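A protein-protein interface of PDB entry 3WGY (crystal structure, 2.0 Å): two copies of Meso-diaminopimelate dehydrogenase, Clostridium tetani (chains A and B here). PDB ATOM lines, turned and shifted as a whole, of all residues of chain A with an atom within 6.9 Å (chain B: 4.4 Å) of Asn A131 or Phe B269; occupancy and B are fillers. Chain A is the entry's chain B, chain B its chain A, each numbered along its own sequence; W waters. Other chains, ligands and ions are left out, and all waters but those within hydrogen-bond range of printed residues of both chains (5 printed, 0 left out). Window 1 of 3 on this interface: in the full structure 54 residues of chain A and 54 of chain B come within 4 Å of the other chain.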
ATOM      1  N   GLY A 126     -14.187   3.693  13.125  1.00  0.00           N
ATOM      2  CA  GLY A 126     -15.437   3.533  13.840  1.00  0.00           C
ATOM      3  C   GLY A 126     -15.233   3.648  15.337  1.00  0.00           C
ATOM      4  O   GLY A 126     -14.874   4.713  15.842  1.00  0.00           O
ATOM      5  N   LEU A 127     -15.444   2.547  16.053  1.00  0.00           N
ATOM      6  CA  LEU A 127     -15.292   2.573  17.503  1.00  0.00           C
ATOM      7  C   LEU A 127     -13.880   2.953  17.949  1.00  0.00           C
ATOM      8  O   LEU A 127     -13.714   3.716  18.899  1.00  0.00           O
ATOM      9  CB  LEU A 127     -15.695   1.225  18.099  1.00  0.00           C
ATOM     10  CG  LEU A 127     -17.087   0.753  17.663  1.00  0.00           C
ATOM     11  CD1 LEU A 127     -17.444  -0.519  18.410  1.00  0.00           C
ATOM     12  CD2 LEU A 127     -18.117   1.839  17.945  1.00  0.00           C
ATOM     13  N   PHE A 128     -12.860   2.437  17.275  1.00  0.00           N
ATOM     14  CA  PHE A 128     -11.504   2.780  17.670  1.00  0.00           C
ATOM     15  C   PHE A 128     -11.246   4.268  17.492  1.00  0.00           C
ATOM     16  O   PHE A 128     -10.579   4.893  18.316  1.00  0.00           O
ATOM     17  CB  PHE A 128     -10.487   1.952  16.877  1.00  0.00           C
ATOM     18  CG  PHE A 128     -10.285   0.562  17.418  1.00  0.00           C
ATOM     19  CD1 PHE A 128     -11.136   0.046  18.387  1.00  0.00           C
ATOM     20  CD2 PHE A 128      -9.256  -0.235  16.947  1.00  0.00           C
ATOM     21  CE1 PHE A 128     -10.957  -1.248  18.875  1.00  0.00           C
ATOM     22  CE2 PHE A 128      -9.069  -1.532  17.432  1.00  0.00           C
ATOM     23  CZ  PHE A 128      -9.918  -2.038  18.393  1.00  0.00           C
ATOM     24  N   SER A 129     -11.798   4.833  16.420  1.00  0.00           N
ATOM     25  CA  SER A 129     -11.652   6.250  16.120  1.00  0.00           C
ATOM     26  C   SER A 129     -12.232   7.080  17.260  1.00  0.00           C
ATOM     27  O   SER A 129     -11.607   8.025  17.729  1.00  0.00           O
ATOM     28  CB  SER A 129     -12.397   6.597  14.822  1.00  0.00           C
ATOM     29  OG  SER A 129     -12.101   5.662  13.800  1.00  0.00           O
ATOM     30  N   LEU A 130     -13.434   6.718  17.698  1.00  0.00           N
ATOM     31  CA  LEU A 130     -14.101   7.438  18.777  1.00  0.00           C
ATOM     32  C   LEU A 130     -13.262   7.414  20.042  1.00  0.00           C
ATOM     33  O   LEU A 130     -13.162   8.419  20.749  1.00  0.00           O
ATOM     34  CB  LEU A 130     -15.466   6.814  19.082  1.00  0.00           C
ATOM     35  CG  LEU A 130     -16.602   7.079  18.094  1.00  0.00           C
ATOM     36  CD1 LEU A 130     -17.701   6.032  18.270  1.00  0.00           C
ATOM     37  CD2 LEU A 130     -17.138   8.514  18.316  1.00  0.00           C
ATOM     38  N   ASN A 131     -12.663   6.262  20.332  1.00  0.00           N
ATOM     39  CA  ASN A 131     -11.866   6.146  21.533  1.00  0.00           C
ATOM     40  C   ASN A 131     -10.525   6.843  21.469  1.00  0.00           C
ATOM     41  O   ASN A 131     -10.012   7.265  22.505  1.00  0.00           O
ATOM     42  CB  ASN A 131     -11.720   4.678  21.947  1.00  0.00           C
ATOM     43  CG  ASN A 131     -12.973   4.164  22.640  1.00  0.00           C
ATOM     44  OD1 ASN A 131     -13.905   3.679  21.999  1.00  0.00           O
ATOM     45  ND2 ASN A 131     -13.014   4.309  23.948  1.00  0.00           N
ATOM     46  N   ARG A 132      -9.946   6.974  20.276  1.00  0.00           N
ATOM     47  CA  ARG A 132      -8.681   7.711  20.172  1.00  0.00           C
ATOM     48  C   ARG A 132      -9.057   9.163  20.485  1.00  0.00           C
ATOM     49  O   ARG A 132      -8.388   9.846  21.255  1.00  0.00           O
ATOM     50  CB  ARG A 132      -8.100   7.645  18.752  1.00  0.00           C
ATOM     51  CG  ARG A 132      -7.669   6.269  18.278  1.00  0.00           C
ATOM     52  CD  ARG A 132      -7.129   6.339  16.842  1.00  0.00           C
ATOM     53  NE  ARG A 132      -7.099   5.020  16.223  1.00  0.00           N
ATOM     54  CZ  ARG A 132      -7.930   4.614  15.269  1.00  0.00           C
ATOM     55  NH1 ARG A 132      -8.871   5.414  14.790  1.00  0.00           N
ATOM     56  NH2 ARG A 132      -7.828   3.387  14.806  1.00  0.00           N
ATOM     57  N   LEU A 133     -10.155   9.615  19.888  1.00  0.00           N
ATOM     58  CA  LEU A 133     -10.643  10.973  20.085  1.00  0.00           C
ATOM     59  C   LEU A 133     -10.923  11.262  21.554  1.00  0.00           C
ATOM     60  O   LEU A 133     -10.437  12.249  22.114  1.00  0.00           O
ATOM     61  CB  LEU A 133     -11.918  11.201  19.266  1.00  0.00           C
ATOM     62  CG  LEU A 133     -12.566  12.578  19.446  1.00  0.00           C
ATOM     63  CD1 LEU A 133     -11.522  13.682  19.237  1.00  0.00           C
ATOM     64  CD2 LEU A 133     -13.734  12.723  18.467  1.00  0.00           C
ATOM     65  N   LEU A 134     -11.713  10.392  22.173  1.00  0.00           N
ATOM     66  CA  LEU A 134     -12.049  10.538  23.581  1.00  0.00           C
ATOM     67  C   LEU A 134     -10.775  10.636  24.411  1.00  0.00           C
ATOM     68  O   LEU A 134     -10.637  11.508  25.266  1.00  0.00           O
ATOM     69  CB  LEU A 134     -12.863   9.326  24.056  1.00  0.00           C
ATOM     70  CG  LEU A 134     -13.396   9.409  25.482  1.00  0.00           C
ATOM     71  CD1 LEU A 134     -14.346  10.603  25.563  1.00  0.00           C
ATOM     72  CD2 LEU A 134     -14.106   8.082  25.855  1.00  0.00           C
ATOM     73  N   GLY A 135      -9.836   9.733  24.145  1.00  0.00           N
ATOM     74  CA  GLY A 135      -8.598   9.715  24.895  1.00  0.00           C
ATOM     75  C   GLY A 135      -7.805  11.009  24.842  1.00  0.00           C
ATOM     76  O   GLY A 135      -7.394  11.535  25.882  1.00  0.00           O
ATOM     77  N   GLU A 136      -7.578  11.528  23.641  1.00  0.00           N
ATOM     78  CA  GLU A 136      -6.794  12.751  23.527  1.00  0.00           C
ATOM     79  C   GLU A 136      -7.582  13.983  23.951  1.00  0.00           C
ATOM     80  O   GLU A 136      -6.993  15.024  24.233  1.00  0.00           O
ATOM     81  CB  GLU A 136      -6.221  12.920  22.102  1.00  0.00           C
ATOM     82  CG  GLU A 136      -7.219  13.100  20.971  1.00  0.00           C
ATOM     83  CD  GLU A 136      -6.516  13.359  19.622  1.00  0.00           C
ATOM     84  OE1 GLU A 136      -5.669  12.527  19.222  1.00  0.00           O
ATOM     85  OE2 GLU A 136      -6.809  14.388  18.968  1.00  0.00           O
ATOM     86  N   SER A 137      -8.905  13.865  24.023  1.00  0.00           N
ATOM     87  CA  SER A 137      -9.726  14.997  24.446  1.00  0.00           C
ATOM     88  C   SER A 137      -9.750  15.081  25.962  1.00  0.00           C
ATOM     89  O   SER A 137      -9.618  16.160  26.536  1.00  0.00           O
ATOM     90  CB  SER A 137     -11.156  14.859  23.928  1.00  0.00           C
ATOM     91  OG  SER A 137     -11.201  15.046  22.529  1.00  0.00           O
ATOM     92  N   THR A 144      -1.294   8.218  22.688  1.00  0.00           N
ATOM     93  CA  THR A 144      -2.314   7.256  22.293  1.00  0.00           C
ATOM     94  C   THR A 144      -1.628   6.077  21.632  1.00  0.00           C
ATOM     95  O   THR A 144      -0.698   6.255  20.843  1.00  0.00           O
ATOM     96  CB  THR A 144      -3.310   7.830  21.274  1.00  0.00           C
ATOM     97  OG1 THR A 144      -3.943   8.990  21.821  1.00  0.00           O
ATOM     98  CG2 THR A 144      -4.363   6.792  20.937  1.00  0.00           C
ATOM     99  N   VAL A 253      -7.051   0.300  22.101  1.00  0.00           N
ATOM    100  CA  VAL A 253      -6.845   1.734  21.964  1.00  0.00           C
ATOM    101  C   VAL A 253      -6.559   2.215  23.381  1.00  0.00           C
ATOM    102  O   VAL A 253      -7.447   2.228  24.235  1.00  0.00           O
ATOM    103  CB  VAL A 253      -8.074   2.469  21.408  1.00  0.00           C
ATOM    104  CG1 VAL A 253      -7.790   3.963  21.364  1.00  0.00           C
ATOM    105  CG2 VAL A 253      -8.393   1.959  20.009  1.00  0.00           C
ATOM    106  N   ILE A 254      -5.316   2.611  23.626  1.00  0.00           N
ATOM    107  CA  ILE A 254      -4.905   3.044  24.950  1.00  0.00           C
ATOM    108  C   ILE A 254      -4.390   4.477  25.049  1.00  0.00           C
ATOM    109  O   ILE A 254      -3.511   4.881  24.291  1.00  0.00           O
ATOM    110  CB  ILE A 254      -3.810   2.110  25.478  1.00  0.00           C
ATOM    111  CG1 ILE A 254      -4.345   0.676  25.546  1.00  0.00           C
ATOM    112  CG2 ILE A 254      -3.311   2.600  26.816  1.00  0.00           C
ATOM    113  CD1 ILE A 254      -3.277  -0.351  25.809  1.00  0.00           C
ATOM    114  N   ARG A 255      -4.931   5.244  25.988  1.00  0.00           N
ATOM    115  CA  ARG A 255      -4.465   6.613  26.170  1.00  0.00           C
ATOM    116  C   ARG A 255      -3.746   6.646  27.495  1.00  0.00           C
ATOM    117  O   ARG A 255      -4.342   6.409  28.556  1.00  0.00           O
ATOM    118  CB  ARG A 255      -5.621   7.621  26.175  1.00  0.00           C
ATOM    119  CG  ARG A 255      -5.183   9.091  26.330  1.00  0.00           C
ATOM    120  CD  ARG A 255      -4.447   9.626  25.089  1.00  0.00           C
ATOM    121  NE  ARG A 255      -4.074  11.038  25.224  1.00  0.00           N
ATOM    122  CZ  ARG A 255      -3.355  11.717  24.332  1.00  0.00           C
ATOM    123  NH1 ARG A 255      -2.923  11.117  23.229  1.00  0.00           N
ATOM    124  NH2 ARG A 255      -3.071  13.000  24.541  1.00  0.00           N
ATOM    125  N   MET A 267      -6.557   5.165  30.095  1.00  0.00           N
ATOM    126  CA  MET A 267      -7.851   4.804  29.533  1.00  0.00           C
ATOM    127  C   MET A 267      -7.593   3.733  28.477  1.00  0.00           C
ATOM    128  O   MET A 267      -6.611   3.800  27.718  1.00  0.00           O
ATOM    129  CB  MET A 267      -8.497   6.008  28.858  1.00  0.00           C
ATOM    130  CG  MET A 267      -8.710   7.209  29.771  1.00  0.00           C
ATOM    131  SD  MET A 267      -9.020   8.709  28.793  1.00  0.00           S
ATOM    132  CE  MET A 267     -10.559   8.293  28.018  1.00  0.00           C
ATOM    133  N   GLU A 268      -8.467   2.742  28.419  1.00  0.00           N
ATOM    134  CA  GLU A 268      -8.308   1.680  27.446  1.00  0.00           C
ATOM    135  C   GLU A 268      -9.642   1.200  26.902  1.00  0.00           C
ATOM    136  O   GLU A 268     -10.625   1.115  27.631  1.00  0.00           O
ATOM    137  CB  GLU A 268      -7.549   0.490  28.080  1.00  0.00           C
ATOM    138  CG  GLU A 268      -7.478  -0.739  27.184  1.00  0.00           C
ATOM    139  CD  GLU A 268      -6.617  -1.879  27.738  1.00  0.00           C
ATOM    140  OE1 GLU A 268      -6.687  -2.986  27.167  1.00  0.00           O
ATOM    141  OE2 GLU A 268      -5.873  -1.681  28.719  1.00  0.00           O
ATOM    142  N   PHE A 269      -9.672   0.926  25.604  1.00  0.00           N
ATOM    143  CA  PHE A 269     -10.853   0.380  24.955  1.00  0.00           C
ATOM    144  C   PHE A 269     -10.292  -0.770  24.135  1.00  0.00           C
ATOM    145  O   PHE A 269      -9.258  -0.616  23.481  1.00  0.00           O
ATOM    146  CB  PHE A 269     -11.508   1.391  24.011  1.00  0.00           C
ATOM    147  CG  PHE A 269     -12.710   0.847  23.278  1.00  0.00           C
ATOM    148  CD1 PHE A 269     -13.954   0.773  23.903  1.00  0.00           C
ATOM    149  CD2 PHE A 269     -12.590   0.384  21.975  1.00  0.00           C
ATOM    150  CE1 PHE A 269     -15.066   0.244  23.228  1.00  0.00           C
ATOM    151  CE2 PHE A 269     -13.687  -0.145  21.295  1.00  0.00           C
ATOM    152  CZ  PHE A 269     -14.930  -0.214  21.925  1.00  0.00           C
ATOM    153  N   ASN A 270     -10.935  -1.926  24.180  1.00  0.00           N
ATOM    154  CA  ASN A 270     -10.443  -3.043  23.389  1.00  0.00           C
ATOM    155  C   ASN A 270     -11.586  -3.941  22.967  1.00  0.00           C
ATOM    156  O   ASN A 270     -12.659  -3.920  23.570  1.00  0.00           O
ATOM    157  CB  ASN A 270      -9.358  -3.832  24.149  1.00  0.00           C
ATOM    158  CG  ASN A 270      -9.898  -4.572  25.347  1.00  0.00           C
ATOM    159  OD1 ASN A 270     -10.832  -5.357  25.230  1.00  0.00           O
ATOM    160  ND2 ASN A 270      -9.300  -4.339  26.506  1.00  0.00           N
ATOM    161  N   PHE A 310     -23.973   9.141  21.155  1.00  0.00           N
ATOM    162  CA  PHE A 310     -24.267   7.728  21.363  1.00  0.00           C
ATOM    163  C   PHE A 310     -25.761   7.466  21.566  1.00  0.00           C
ATOM    164  O   PHE A 310     -26.247   6.379  21.269  1.00  0.00           O
ATOM    165  CB  PHE A 310     -23.474   7.190  22.555  1.00  0.00           C
ATOM    166  CG  PHE A 310     -22.023   6.921  22.252  1.00  0.00           C
ATOM    167  CD1 PHE A 310     -21.426   7.416  21.097  1.00  0.00           C
ATOM    168  CD2 PHE A 310     -21.247   6.187  23.141  1.00  0.00           C
ATOM    169  CE1 PHE A 310     -20.077   7.185  20.836  1.00  0.00           C
ATOM    170  CE2 PHE A 310     -19.898   5.949  22.888  1.00  0.00           C
ATOM    171  CZ  PHE A 310     -19.311   6.446  21.740  1.00  0.00           C
ATOM    172  N   LEU B 127     -18.076   8.704  31.441  1.00  0.00           N
ATOM    173  CA  LEU B 127     -17.431   7.780  30.516  1.00  0.00           C
ATOM    174  C   LEU B 127     -17.984   6.357  30.577  1.00  0.00           C
ATOM    175  O   LEU B 127     -18.213   5.734  29.545  1.00  0.00           O
ATOM    176  CB  LEU B 127     -15.911   7.765  30.746  1.00  0.00           C
ATOM    177  CG  LEU B 127     -15.225   9.138  30.739  1.00  0.00           C
ATOM    178  CD1 LEU B 127     -13.712   8.945  30.554  1.00  0.00           C
ATOM    179  CD2 LEU B 127     -15.792  10.008  29.618  1.00  0.00           C
ATOM    180  N   PHE B 128     -18.190   5.838  31.779  1.00  0.00           N
ATOM    181  CA  PHE B 128     -18.721   4.493  31.920  1.00  0.00           C
ATOM    182  C   PHE B 128     -20.139   4.412  31.366  1.00  0.00           C
ATOM    183  O   PHE B 128     -20.515   3.407  30.771  1.00  0.00           O
ATOM    184  CB  PHE B 128     -18.699   4.062  33.391  1.00  0.00           C
ATOM    185  CG  PHE B 128     -17.376   3.503  33.839  1.00  0.00           C
ATOM    186  CD1 PHE B 128     -16.221   3.715  33.092  1.00  0.00           C
ATOM    187  CD2 PHE B 128     -17.283   2.774  35.023  1.00  0.00           C
ATOM    188  CE1 PHE B 128     -14.992   3.208  33.519  1.00  0.00           C
ATOM    189  CE2 PHE B 128     -16.067   2.263  35.458  1.00  0.00           C
ATOM    190  CZ  PHE B 128     -14.914   2.481  34.701  1.00  0.00           C
ATOM    191  N   ASN B 131     -20.036   4.069  27.689  1.00  0.00           N
ATOM    192  CA  ASN B 131     -19.662   2.739  27.239  1.00  0.00           C
ATOM    193  C   ASN B 131     -20.713   1.687  27.516  1.00  0.00           C
ATOM    194  O   ASN B 131     -20.772   0.665  26.829  1.00  0.00           O
ATOM    195  CB  ASN B 131     -18.317   2.356  27.812  1.00  0.00           C
ATOM    196  CG  ASN B 131     -17.191   3.053  27.083  1.00  0.00           C
ATOM    197  OD1 ASN B 131     -16.809   4.176  27.416  1.00  0.00           O
ATOM    198  ND2 ASN B 131     -16.692   2.409  26.046  1.00  0.00           N
ATOM    199  N   GLY B 251     -11.865   1.264  36.995  1.00  0.00           N
ATOM    200  CA  GLY B 251     -13.018   0.405  36.817  1.00  0.00           C
ATOM    201  C   GLY B 251     -13.053  -0.203  35.444  1.00  0.00           C
ATOM    202  O   GLY B 251     -12.194   0.081  34.603  1.00  0.00           O
ATOM    203  N   PHE B 252     -14.067  -1.030  35.217  1.00  0.00           N
ATOM    204  CA  PHE B 252     -14.222  -1.721  33.957  1.00  0.00           C
ATOM    205  C   PHE B 252     -15.678  -1.750  33.527  1.00  0.00           C
ATOM    206  O   PHE B 252     -16.579  -1.856  34.363  1.00  0.00           O
ATOM    207  CB  PHE B 252     -13.733  -3.174  34.086  1.00  0.00           C
ATOM    208  CG  PHE B 252     -12.378  -3.312  34.718  1.00  0.00           C
ATOM    209  CD1 PHE B 252     -12.205  -3.101  36.078  1.00  0.00           C
ATOM    210  CD2 PHE B 252     -11.271  -3.619  33.946  1.00  0.00           C
ATOM    211  CE1 PHE B 252     -10.940  -3.189  36.668  1.00  0.00           C
ATOM    212  CE2 PHE B 252     -10.002  -3.709  34.520  1.00  0.00           C
ATOM    213  CZ  PHE B 252      -9.835  -3.493  35.885  1.00  0.00           C
ATOM    214  N   VAL B 253     -15.904  -1.631  32.223  1.00  0.00           N
ATOM    215  CA  VAL B 253     -17.248  -1.726  31.669  1.00  0.00           C
ATOM    216  C   VAL B 253     -17.115  -2.734  30.537  1.00  0.00           C
ATOM    217  O   VAL B 253     -16.512  -2.449  29.505  1.00  0.00           O
ATOM    218  CB  VAL B 253     -17.769  -0.393  31.107  1.00  0.00           C
ATOM    219  CG1 VAL B 253     -19.166  -0.593  30.516  1.00  0.00           C
ATOM    220  CG2 VAL B 253     -17.809   0.654  32.202  1.00  0.00           C
ATOM    221  N   GLU B 268     -14.690  -3.968  25.752  1.00  0.00           N
ATOM    222  CA  GLU B 268     -14.264  -3.509  27.068  1.00  0.00           C
ATOM    223  C   GLU B 268     -13.699  -2.096  27.084  1.00  0.00           C
ATOM    224  O   GLU B 268     -12.967  -1.691  26.182  1.00  0.00           O
ATOM    225  CB  GLU B 268     -13.213  -4.449  27.665  1.00  0.00           C
ATOM    226  CG  GLU B 268     -12.863  -4.091  29.103  1.00  0.00           C
ATOM    227  CD  GLU B 268     -11.806  -4.996  29.719  1.00  0.00           C
ATOM    228  OE1 GLU B 268     -11.807  -6.203  29.424  1.00  0.00           O
ATOM    229  OE2 GLU B 268     -10.989  -4.503  30.523  1.00  0.00           O
ATOM    230  N   PHE B 269     -14.058  -1.353  28.121  1.00  0.00           N
ATOM    231  CA  PHE B 269     -13.549  -0.004  28.327  1.00  0.00           C
ATOM    232  C   PHE B 269     -13.108  -0.011  29.771  1.00  0.00           C
ATOM    233  O   PHE B 269     -13.850  -0.485  30.626  1.00  0.00           O
ATOM    234  CB  PHE B 269     -14.640   1.047  28.178  1.00  0.00           C
ATOM    235  CG  PHE B 269     -14.186   2.437  28.532  1.00  0.00           C
ATOM    236  CD1 PHE B 269     -13.507   3.222  27.597  1.00  0.00           C
ATOM    237  CD2 PHE B 269     -14.406   2.952  29.807  1.00  0.00           C
ATOM    238  CE1 PHE B 269     -13.056   4.498  27.924  1.00  0.00           C
ATOM    239  CE2 PHE B 269     -13.954   4.233  30.151  1.00  0.00           C
ATOM    240  CZ  PHE B 269     -13.278   5.011  29.206  1.00  0.00           C
ATOM    241  N   ASN B 270     -11.919   0.492  30.065  1.00  0.00           N
ATOM    242  CA  ASN B 270     -11.501   0.507  31.449  1.00  0.00           C
ATOM    243  C   ASN B 270     -10.586   1.681  31.780  1.00  0.00           C
ATOM    244  O   ASN B 270     -10.004   2.296  30.885  1.00  0.00           O
ATOM    245  CB  ASN B 270     -10.858  -0.843  31.822  1.00  0.00           C
ATOM    246  CG  ASN B 270      -9.484  -1.035  31.222  1.00  0.00           C
ATOM    247  OD1 ASN B 270      -8.602  -0.212  31.405  1.00  0.00           O
ATOM    248  ND2 ASN B 270      -9.295  -2.142  30.516  1.00  0.00           N
ATOM    249  N   LEU B 271     -10.504   2.000  33.068  1.00  0.00           N
ATOM    250  CA  LEU B 271      -9.699   3.110  33.570  1.00  0.00           C
ATOM    251  C   LEU B 271      -8.805   2.677  34.722  1.00  0.00           C
ATOM    252  O   LEU B 271      -9.223   1.910  35.596  1.00  0.00           O
ATOM    253  CB  LEU B 271     -10.597   4.247  34.081  1.00  0.00           C
ATOM    254  CG  LEU B 271     -11.590   4.926  33.129  1.00  0.00           C
ATOM    255  CD1 LEU B 271     -12.409   5.934  33.910  1.00  0.00           C
ATOM    256  CD2 LEU B 271     -10.825   5.640  31.989  1.00  0.00           C
HETATM  257  O   HOH W   1     -15.715   4.491  24.463  1.00  0.00           O
HETATM  258  O   HOH W   2     -12.096  -7.570  27.239  1.00  0.00           O
HETATM  259  O   HOH W   3      -5.654  -0.462  30.928  1.00  0.00           O
HETATM  260  O   HOH W   4      -8.703  -6.307  28.979  1.00  0.00           O
HETATM  261  O   HOH W   5      -7.039  -4.403  29.728  1.00  0.00           O
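Asn A131 touches Phe B269, and with the chains exchanged Phe A269 touches Asn B131.
Glu A268 touches its own counterpart, Glu B268.
Glu A268 touches Phe B269, and with the chains exchanged Phe A269 touches Glu B268.
Glu A268 touches Asn B270, and with the chains exchanged Asn A270 touches Glu B268.
Of chain B, only Phe B269 (3.8 Å) comes within 4 Å of Asn A131.
Of the printed residues of chain A, Asn B270 touches Met A267 and Glu A268.
Of the printed residues of chain B, Met A267 touches Asn B270 and Leu B271.
Arg A132 touches none of the printed residues of chain B.
Phe A128 touches none of the printed residues of chain B.
The nearest printed residue of chain B that does not touch Asn A131 is Asn B131 (4.6 Å).
The nearest residue of chain A that does not touch Phe B269 is Leu A134 (4.3 Å).
Asn A131 touches Phe B269.
Met A267 touches Asn B270.
CD2 of Leu B271 touches CG of Met A267, 3.4 Å away.
Glu B268 touches Glu A268.
CA of Phe B269 touches O of Glu A268, 3.2 Å away.
Asn B131 touches Phe A269 (ND2 to CD1, 3.8 Å).
CA of Phe A269 touches O of Glu B268, at 3.2 Å.
Of the 21 printed residues of chain A, 5 touch a printed residue of chain B.
Hydrophobic or aromatic side chains of chain A within 4 Å of the printed part of chain B: Met A267 and Phe A269.
Hydrophobic or aromatic side chains of chain B within 4 Å of the printed part of chain A: Phe B269 and Leu B271.
The backbone carbonyl oxygen (O) of Phe A269 sits at hydrogen-bond distance from the backbone NH (N) of Val A253, 2.8 Å away.
The backbone carbonyl oxygen (O) of Leu B127 sits close to the side-chain amide oxygen (OD1) of Asn B131 (3.0 Å).
N of Arg A255 lies within hydrogen-bond range of O of Met A267.
The backbone carbonyl oxygen (O) of Leu A127 lies close to the side-chain amide oxygen (OD1) of Asn A131, at 3.1 Å.
N of Val B253 sits at hydrogen-bond distance from O of Phe B269.
The side-chain carboxylate (OE1) of Glu A268 sits at hydrogen-bond distance from the side-chain amide nitrogen (ND2) of Asn A270.
The backbone NH of Asn B270 lies within hydrogen-bond range of the backbone carbonyl oxygen of Glu A268.
The backbone carbonyl oxygen of Glu B268 is in hydrogen-bond range of the backbone NH of Asn A270 (2.9 Å).
Water W3 bridges the side-chain carboxylate (OE2) of Glu A268 and the side-chain amide oxygen (OD1) of Asn B270.
Water W2 bridges OE1 of Glu B268 and OD1 of Asn A270.
Water W1 bridges ND2 of Asn A131 (2.8 Å) and ND2 of Asn B131 (2.8 Å).
Water W5 lies within hydrogen-bond range of the side-chain carboxylate (OE1) of Glu A268 and the side-chain amide nitrogen (ND2) of Asn B270.
Water W4 bridges the side-chain carboxylate (OE1) of Glu B268 and the side-chain amide nitrogen (ND2) of Asn A270.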
